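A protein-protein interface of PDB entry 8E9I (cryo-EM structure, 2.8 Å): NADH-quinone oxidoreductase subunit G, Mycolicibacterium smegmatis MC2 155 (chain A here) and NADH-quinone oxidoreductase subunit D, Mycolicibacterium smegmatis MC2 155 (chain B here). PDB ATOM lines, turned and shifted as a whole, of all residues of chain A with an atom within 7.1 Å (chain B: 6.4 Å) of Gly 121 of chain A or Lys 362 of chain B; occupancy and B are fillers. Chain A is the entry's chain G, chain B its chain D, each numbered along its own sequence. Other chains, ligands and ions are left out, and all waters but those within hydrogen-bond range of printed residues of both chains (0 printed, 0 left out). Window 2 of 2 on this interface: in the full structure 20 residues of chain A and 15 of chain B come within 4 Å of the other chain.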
ATOM      1  N   CYS A 114      15.235  19.618  24.160  1.00  0.00           N
ATOM      2  CA  CYS A 114      14.697  18.937  25.332  1.00  0.00           C
ATOM      3  C   CYS A 114      15.456  17.665  25.670  1.00  0.00           C
ATOM      4  O   CYS A 114      15.774  17.469  26.853  1.00  0.00           O
ATOM      5  CB  CYS A 114      13.206  18.643  25.123  1.00  0.00           C
ATOM      6  SG  CYS A 114      12.213  20.106  24.810  1.00  0.00           S
ATOM      7  N   CYS A 117      18.666  19.110  27.070  1.00  0.00           N
ATOM      8  CA  CYS A 117      18.528  20.115  28.113  1.00  0.00           C
ATOM      9  C   CYS A 117      18.397  19.454  29.477  1.00  0.00           C
ATOM     10  O   CYS A 117      17.568  18.561  29.666  1.00  0.00           O
ATOM     11  CB  CYS A 117      17.307  20.980  27.840  1.00  0.00           C
ATOM     12  SG  CYS A 117      16.957  22.150  29.133  1.00  0.00           S
ATOM     13  N   ASP A 118      19.197  19.910  30.440  1.00  0.00           N
ATOM     14  CA  ASP A 118      19.101  19.356  31.786  1.00  0.00           C
ATOM     15  C   ASP A 118      17.728  19.590  32.387  1.00  0.00           C
ATOM     16  O   ASP A 118      17.240  18.761  33.161  1.00  0.00           O
ATOM     17  CB  ASP A 118      20.172  19.961  32.687  1.00  0.00           C
ATOM     18  CG  ASP A 118      21.555  19.462  32.351  1.00  0.00           C
ATOM     19  OD1 ASP A 118      21.682  18.268  32.019  1.00  0.00           O
ATOM     20  OD2 ASP A 118      22.510  20.258  32.421  1.00  0.00           O
ATOM     21  N   LYS A 119      17.085  20.701  32.042  1.00  0.00           N
ATOM     22  CA  LYS A 119      15.778  21.004  32.598  1.00  0.00           C
ATOM     23  C   LYS A 119      14.692  20.069  32.082  1.00  0.00           C
ATOM     24  O   LYS A 119      13.575  20.103  32.603  1.00  0.00           O
ATOM     25  CB  LYS A 119      15.420  22.459  32.300  1.00  0.00           C
ATOM     26  CG  LYS A 119      14.217  22.963  33.059  1.00  0.00           C
ATOM     27  CD  LYS A 119      14.491  23.217  34.527  1.00  0.00           C
ATOM     28  CE  LYS A 119      15.137  24.557  34.765  1.00  0.00           C
ATOM     29  NZ  LYS A 119      15.136  24.902  36.208  1.00  0.00           N
ATOM     30  N   GLY A 120      14.987  19.231  31.094  1.00  0.00           N
ATOM     31  CA  GLY A 120      13.985  18.338  30.549  1.00  0.00           C
ATOM     32  C   GLY A 120      13.334  17.483  31.609  1.00  0.00           C
ATOM     33  O   GLY A 120      14.024  16.881  32.435  1.00  0.00           O
ATOM     34  N   GLY A 121      12.011  17.425  31.601  1.00  0.00           N
ATOM     35  CA  GLY A 121      11.278  16.687  32.621  1.00  0.00           C
ATOM     36  C   GLY A 121      10.862  17.542  33.781  1.00  0.00           C
ATOM     37  O   GLY A 121       9.783  17.340  34.346  1.00  0.00           O
ATOM     38  N   GLU A 122      11.701  18.497  34.167  1.00  0.00           N
ATOM     39  CA  GLU A 122      11.344  19.464  35.192  1.00  0.00           C
ATOM     40  C   GLU A 122      11.162  20.864  34.633  1.00  0.00           C
ATOM     41  O   GLU A 122      11.236  21.828  35.399  1.00  0.00           O
ATOM     42  CB  GLU A 122      12.408  19.490  36.286  1.00  0.00           C
ATOM     43  N   CYS A 123      10.945  21.001  33.335  1.00  0.00           N
ATOM     44  CA  CYS A 123      10.913  22.315  32.714  1.00  0.00           C
ATOM     45  C   CYS A 123       9.519  22.914  32.809  1.00  0.00           C
ATOM     46  O   CYS A 123       8.568  22.322  32.295  1.00  0.00           O
ATOM     47  CB  CYS A 123      11.330  22.220  31.259  1.00  0.00           C
ATOM     48  SG  CYS A 123      11.668  23.803  30.498  1.00  0.00           S
ATOM     49  N   PRO A 124       9.350  24.069  33.449  1.00  0.00           N
ATOM     50  CA  PRO A 124       8.054  24.749  33.361  1.00  0.00           C
ATOM     51  C   PRO A 124       7.658  25.090  31.943  1.00  0.00           C
ATOM     52  O   PRO A 124       6.464  25.087  31.629  1.00  0.00           O
ATOM     53  CB  PRO A 124       8.266  26.000  34.217  1.00  0.00           C
ATOM     54  CG  PRO A 124       9.300  25.606  35.180  1.00  0.00           C
ATOM     55  CD  PRO A 124      10.224  24.697  34.450  1.00  0.00           C
ATOM     56  N   GLN A 126       8.226  23.269  29.183  1.00  0.00           N
ATOM     57  CA  GLN A 126       7.620  22.061  28.634  1.00  0.00           C
ATOM     58  C   GLN A 126       6.215  21.865  29.172  1.00  0.00           C
ATOM     59  O   GLN A 126       5.267  21.638  28.413  1.00  0.00           O
ATOM     60  CB  GLN A 126       8.461  20.838  28.979  1.00  0.00           C
ATOM     61  CG  GLN A 126       9.686  20.636  28.150  1.00  0.00           C
ATOM     62  CD  GLN A 126      10.370  19.337  28.494  1.00  0.00           C
ATOM     63  OE1 GLN A 126      10.522  19.000  29.664  1.00  0.00           O
ATOM     64  NE2 GLN A 126      10.776  18.592  27.480  1.00  0.00           N
ATOM     65  N   ASN A 127       6.071  21.916  30.493  1.00  0.00           N
ATOM     66  CA  ASN A 127       4.794  21.594  31.108  1.00  0.00           C
ATOM     67  C   ASN A 127       3.715  22.566  30.665  1.00  0.00           C
ATOM     68  O   ASN A 127       2.585  22.164  30.360  1.00  0.00           O
ATOM     69  CB  ASN A 127       4.950  21.609  32.623  1.00  0.00           C
ATOM     70  CG  ASN A 127       6.123  20.783  33.085  1.00  0.00           C
ATOM     71  OD1 ASN A 127       6.546  19.855  32.402  1.00  0.00           O
ATOM     72  ND2 ASN A 127       6.673  21.129  34.236  1.00  0.00           N
ATOM     73  N   MET A 130       2.676  22.043  27.121  1.00  0.00           N
ATOM     74  CA  MET A 130       1.709  20.955  27.055  1.00  0.00           C
ATOM     75  C   MET A 130       0.323  21.438  27.453  1.00  0.00           C
ATOM     76  O   MET A 130      -0.658  21.220  26.735  1.00  0.00           O
ATOM     77  CB  MET A 130       2.145  19.803  27.958  1.00  0.00           C
ATOM     78  CG  MET A 130       3.218  18.909  27.389  1.00  0.00           C
ATOM     79  SD  MET A 130       2.914  18.466  25.676  1.00  0.00           S
ATOM     80  CE  MET A 130       2.289  16.807  25.877  1.00  0.00           C
ATOM     81  N   ARG A 228      18.324  12.815  34.904  1.00  0.00           N
ATOM     82  CA  ARG A 228      16.994  13.324  34.624  1.00  0.00           C
ATOM     83  C   ARG A 228      16.107  13.141  35.840  1.00  0.00           C
ATOM     84  O   ARG A 228      16.373  12.295  36.699  1.00  0.00           O
ATOM     85  CB  ARG A 228      16.373  12.605  33.424  1.00  0.00           C
ATOM     86  CG  ARG A 228      17.306  12.379  32.250  1.00  0.00           C
ATOM     87  CD  ARG A 228      18.029  13.639  31.818  1.00  0.00           C
ATOM     88  NE  ARG A 228      17.140  14.639  31.247  1.00  0.00           N
ATOM     89  CZ  ARG A 228      16.943  14.819  29.949  1.00  0.00           C
ATOM     90  NH1 ARG A 228      17.485  14.020  29.048  1.00  0.00           N
ATOM     91  NH2 ARG A 228      16.184  15.828  29.543  1.00  0.00           N
ATOM     92  N   PRO A 229      15.017  13.902  35.937  1.00  0.00           N
ATOM     93  CA  PRO A 229      14.232  13.888  37.179  1.00  0.00           C
ATOM     94  C   PRO A 229      13.836  12.497  37.625  1.00  0.00           C
ATOM     95  O   PRO A 229      13.880  12.196  38.822  1.00  0.00           O
ATOM     96  CB  PRO A 229      13.005  14.729  36.813  1.00  0.00           C
ATOM     97  CG  PRO A 229      13.472  15.620  35.745  1.00  0.00           C
ATOM     98  CD  PRO A 229      14.475  14.852  34.956  1.00  0.00           C
ATOM     99  N   PHE A 230      13.466  11.628  36.694  1.00  0.00           N
ATOM    100  CA  PHE A 230      13.056  10.284  37.063  1.00  0.00           C
ATOM    101  C   PHE A 230      14.187   9.463  37.661  1.00  0.00           C
ATOM    102  O   PHE A 230      13.911   8.472  38.340  1.00  0.00           O
ATOM    103  CB  PHE A 230      12.496   9.575  35.838  1.00  0.00           C
ATOM    104  CG  PHE A 230      13.521   8.828  35.058  1.00  0.00           C
ATOM    105  CD1 PHE A 230      14.287   9.472  34.113  1.00  0.00           C
ATOM    106  CD2 PHE A 230      13.722   7.485  35.269  1.00  0.00           C
ATOM    107  CE1 PHE A 230      15.231   8.787  33.395  1.00  0.00           C
ATOM    108  CE2 PHE A 230      14.661   6.802  34.556  1.00  0.00           C
ATOM    109  CZ  PHE A 230      15.418   7.455  33.616  1.00  0.00           C
ATOM    110  N   LEU B 357       8.470  18.323  19.692  1.00  0.00           N
ATOM    111  CA  LEU B 357       9.470  17.768  20.593  1.00  0.00           C
ATOM    112  C   LEU B 357       8.965  17.754  22.025  1.00  0.00           C
ATOM    113  O   LEU B 357       9.134  16.762  22.740  1.00  0.00           O
ATOM    114  CB  LEU B 357      10.761  18.572  20.492  1.00  0.00           C
ATOM    115  CG  LEU B 357      11.935  18.088  21.340  1.00  0.00           C
ATOM    116  CD1 LEU B 357      12.250  16.637  21.052  1.00  0.00           C
ATOM    117  CD2 LEU B 357      13.147  18.948  21.072  1.00  0.00           C
ATOM    118  N   ILE B 358       8.347  18.847  22.465  1.00  0.00           N
ATOM    119  CA  ILE B 358       7.855  18.910  23.835  1.00  0.00           C
ATOM    120  C   ILE B 358       6.801  17.841  24.059  1.00  0.00           C
ATOM    121  O   ILE B 358       6.779  17.176  25.098  1.00  0.00           O
ATOM    122  CB  ILE B 358       7.307  20.311  24.150  1.00  0.00           C
ATOM    123  CG1 ILE B 358       8.453  21.311  24.234  1.00  0.00           C
ATOM    124  CG2 ILE B 358       6.523  20.285  25.447  1.00  0.00           C
ATOM    125  CD1 ILE B 358       8.004  22.746  24.329  1.00  0.00           C
ATOM    126  N   HIS B 359       5.896  17.674  23.096  1.00  0.00           N
ATOM    127  CA  HIS B 359       4.839  16.688  23.256  1.00  0.00           C
ATOM    128  C   HIS B 359       5.402  15.279  23.289  1.00  0.00           C
ATOM    129  O   HIS B 359       5.005  14.468  24.130  1.00  0.00           O
ATOM    130  CB  HIS B 359       3.814  16.840  22.142  1.00  0.00           C
ATOM    131  CG  HIS B 359       2.879  17.983  22.358  1.00  0.00           C
ATOM    132  ND1 HIS B 359       3.280  19.297  22.276  1.00  0.00           N
ATOM    133  CD2 HIS B 359       1.563  18.012  22.672  1.00  0.00           C
ATOM    134  CE1 HIS B 359       2.253  20.086  22.522  1.00  0.00           C
ATOM    135  NE2 HIS B 359       1.199  19.331  22.766  1.00  0.00           N
ATOM    136  N   HIS B 360       6.330  14.964  22.390  1.00  0.00           N
ATOM    137  CA  HIS B 360       6.963  13.653  22.440  1.00  0.00           C
ATOM    138  C   HIS B 360       7.607  13.426  23.800  1.00  0.00           C
ATOM    139  O   HIS B 360       7.354  12.416  24.469  1.00  0.00           O
ATOM    140  CB  HIS B 360       8.002  13.535  21.330  1.00  0.00           C
ATOM    141  CG  HIS B 360       8.782  12.264  21.374  1.00  0.00           C
ATOM    142  ND1 HIS B 360       8.372  11.119  20.729  1.00  0.00           N
ATOM    143  CD2 HIS B 360       9.936  11.948  22.004  1.00  0.00           C
ATOM    144  CE1 HIS B 360       9.248  10.157  20.944  1.00  0.00           C
ATOM    145  NE2 HIS B 360      10.206  10.632  21.718  1.00  0.00           N
ATOM    146  N   PHE B 361       8.413  14.389  24.240  1.00  0.00           N
ATOM    147  CA  PHE B 361       9.146  14.261  25.490  1.00  0.00           C
ATOM    148  C   PHE B 361       8.196  14.036  26.661  1.00  0.00           C
ATOM    149  O   PHE B 361       8.400  13.136  27.480  1.00  0.00           O
ATOM    150  CB  PHE B 361       9.987  15.523  25.687  1.00  0.00           C
ATOM    151  CG  PHE B 361      10.997  15.431  26.785  1.00  0.00           C
ATOM    152  CD1 PHE B 361      10.609  15.399  28.106  1.00  0.00           C
ATOM    153  CD2 PHE B 361      12.341  15.403  26.491  1.00  0.00           C
ATOM    154  CE1 PHE B 361      11.540  15.329  29.108  1.00  0.00           C
ATOM    155  CE2 PHE B 361      13.275  15.336  27.488  1.00  0.00           C
ATOM    156  CZ  PHE B 361      12.875  15.296  28.797  1.00  0.00           C
ATOM    157  N   LYS B 362       7.140  14.844  26.754  1.00  0.00           N
ATOM    158  CA  LYS B 362       6.278  14.789  27.928  1.00  0.00           C
ATOM    159  C   LYS B 362       5.352  13.583  27.895  1.00  0.00           C
ATOM    160  O   LYS B 362       5.094  12.971  28.935  1.00  0.00           O
ATOM    161  CB  LYS B 362       5.468  16.078  28.043  1.00  0.00           C
ATOM    162  CG  LYS B 362       6.295  17.301  28.389  1.00  0.00           C
ATOM    163  CD  LYS B 362       7.031  17.166  29.711  1.00  0.00           C
ATOM    164  CE  LYS B 362       6.100  16.830  30.850  1.00  0.00           C
ATOM    165  NZ  LYS B 362       6.764  17.038  32.161  1.00  0.00           N
ATOM    166  N   LEU B 363       4.812  13.238  26.724  1.00  0.00           N
ATOM    167  CA  LEU B 363       3.910  12.099  26.645  1.00  0.00           C
ATOM    168  C   LEU B 363       4.657  10.792  26.808  1.00  0.00           C
ATOM    169  O   LEU B 363       4.066   9.788  27.215  1.00  0.00           O
ATOM    170  CB  LEU B 363       3.171  12.105  25.314  1.00  0.00           C
ATOM    171  CG  LEU B 363       2.275  13.319  25.118  1.00  0.00           C
ATOM    172  CD1 LEU B 363       1.814  13.414  23.685  1.00  0.00           C
ATOM    173  CD2 LEU B 363       1.095  13.253  26.056  1.00  0.00           C
ATOM    174  N   VAL B 364       5.947  10.779  26.488  1.00  0.00           N
ATOM    175  CA  VAL B 364       6.728   9.566  26.656  1.00  0.00           C
ATOM    176  C   VAL B 364       7.201   9.434  28.095  1.00  0.00           C
ATOM    177  O   VAL B 364       7.136   8.352  28.687  1.00  0.00           O
ATOM    178  CB  VAL B 364       7.893   9.574  25.657  1.00  0.00           C
ATOM    179  CG1 VAL B 364       8.942   8.570  26.033  1.00  0.00           C
ATOM    180  CG2 VAL B 364       7.369   9.281  24.270  1.00  0.00           C
ATOM    181  N   THR B 365       7.684  10.524  28.679  1.00  0.00           N
ATOM    182  CA  THR B 365       8.276  10.483  30.008  1.00  0.00           C
ATOM    183  C   THR B 365       7.243  10.589  31.117  1.00  0.00           C
ATOM    184  O   THR B 365       7.047   9.646  31.886  1.00  0.00           O
ATOM    185  CB  THR B 365       9.284  11.614  30.149  1.00  0.00           C
ATOM    186  OG1 THR B 365       8.626  12.870  29.955  1.00  0.00           O
ATOM    187  CG2 THR B 365      10.386  11.457  29.140  1.00  0.00           C
ATOM    188  N   GLU B 366       6.580  11.739  31.213  1.00  0.00           N
ATOM    189  CA  GLU B 366       5.552  11.901  32.232  1.00  0.00           C
ATOM    190  C   GLU B 366       4.285  11.162  31.841  1.00  0.00           C
ATOM    191  O   GLU B 366       3.658  10.509  32.681  1.00  0.00           O
ATOM    192  CB  GLU B 366       5.257  13.383  32.452  1.00  0.00           C
ATOM    193  N   GLY B 367       3.908  11.239  30.574  1.00  0.00           N
ATOM    194  CA  GLY B 367       2.679  10.651  30.091  1.00  0.00           C
ATOM    195  C   GLY B 367       1.483  11.534  30.381  1.00  0.00           C
ATOM    196  O   GLY B 367       1.528  12.467  31.184  1.00  0.00           O
ATOM    197  N   ILE B 368       0.385  11.226  29.694  1.00  0.00           N
ATOM    198  CA  ILE B 368      -0.847  11.955  29.926  1.00  0.00           C
ATOM    199  C   ILE B 368      -1.201  11.908  31.406  1.00  0.00           C
ATOM    200  O   ILE B 368      -0.867  10.960  32.125  1.00  0.00           O
ATOM    201  CB  ILE B 368      -1.985  11.370  29.079  1.00  0.00           C
ATOM    202  CG1 ILE B 368      -2.198   9.898  29.431  1.00  0.00           C
ATOM    203  CG2 ILE B 368      -1.651  11.490  27.618  1.00  0.00           C
ATOM    204  CD1 ILE B 368      -3.419   9.299  28.801  1.00  0.00           C
ATOM    205  N   ARG B 369      -1.881  12.949  31.866  1.00  0.00           N
ATOM    206  CA  ARG B 369      -2.489  12.949  33.184  1.00  0.00           C
ATOM    207  C   ARG B 369      -3.997  12.933  33.007  1.00  0.00           C
ATOM    208  O   ARG B 369      -4.557  13.753  32.277  1.00  0.00           O
ATOM    209  CB  ARG B 369      -2.048  14.156  34.016  1.00  0.00           C
ATOM    210  CG  ARG B 369      -2.288  15.497  33.384  1.00  0.00           C
ATOM    211  CD  ARG B 369      -1.699  16.601  34.248  1.00  0.00           C
ATOM    212  NE  ARG B 369      -0.248  16.482  34.350  1.00  0.00           N
ATOM    213  CZ  ARG B 369       0.482  16.914  35.370  1.00  0.00           C
ATOM    214  NH1 ARG B 369      -0.071  17.498  36.420  1.00  0.00           N
ATOM    215  NH2 ARG B 369       1.802  16.764  35.330  1.00  0.00           N
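A ring nitrogen (NE2) of His 359 of chain B lies close to the side-chain sulfur (SD) of Met 130 of chain A. NZ of Lys 362 of chain B sits at hydrogen-bond distance from OD1 of Asn 127 of chain A (2.8 Å).
The backbone carbonyl oxygen (O) of Phe 361 of chain B sits at hydrogen-bond distance from the side-chain hydroxyl (OG1) of Thr 365 of chain B (2.5 Å). O of Cys 114 of chain A lies within hydrogen-bond range of NH2 of Arg 228 of chain A (3.2 Å). The guanidinium group (NH2) of Arg 228 of chain A sits at hydrogen-bond distance from the backbone carbonyl oxygen (O) of Cys 117 of chain A. The backbone NH of Gly 121 of chain A is in hydrogen-bond range of the side-chain amide oxygen of Gln 126 of chain A (2.9 Å). The backbone NH of Gln 126 of chain A sits close to the side-chain sulfur of Cys 123 of chain A, 3.7 Å away. O of Cys 123 of chain A lies within hydrogen-bond range of ND2 of Asn 127 of chain A.
Among the printed residues, pairs that only touch across the chains: Gln 126 of chain A with Phe 361 of chain B (3.2 Å), Gly 121 of chain A with Phe 361 of chain B (3.3 Å), Cys 114 of chain A with Phe 361 of chain B (3.3 Å), Arg 228 of chain A with Phe 361 of chain B (3.4 Å), Gln 126 of chain A with Ile 358 of chain B (3.5 Å), Met 130 of chain A with Leu 363 of chain B (3.6 Å), Gly 120 of chain A with Phe 361 of chain B (3.6 Å), Met 130 of chain A with Lys 362 of chain B (3.6 Å), Gly 121 of chain A with Lys 362 of chain B (3.7 Å), Cys 114 of chain A with Leu 357 of chain B (3.8 Å), Gln 126 of chain A with Lys 362 of chain B (3.9 Å) and Cys 114 of chain A with Ile 358 of chain B (3.99 Å).
Of chain B, only Phe 361 (3.3 Å) and Lys 362 (3.7 Å) come within 4 Å of Gly 121 of chain A. Of the printed residues of chain B, Gln 126 of chain A touches Ile 358, Phe 361 and Lys 362. Of the printed residues of chain A, Ile 358 of chain B touches Cys 114 (3.99 Å) and Gln 126 (3.5 Å). Gly 367 of chain B touches none of the printed residues of chain A. Pro 229 of chain A touches none of the printed residues of chain B. The nearest printed residue of chain B that does not touch Gln 126 of chain A is Leu 357 of chain B (5.3 Å).
Hydrophobic or aromatic side chains of chain A within 4 Å of the printed part of chain B: Met 130. Of the 13 printed residues of chain B, 6 touch a printed residue of chain A. Hydrophobic or aromatic side chains of chain B that line the printed part of chain A: Leu 357, Ile 358, His 359, Phe 361 and Leu 363.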
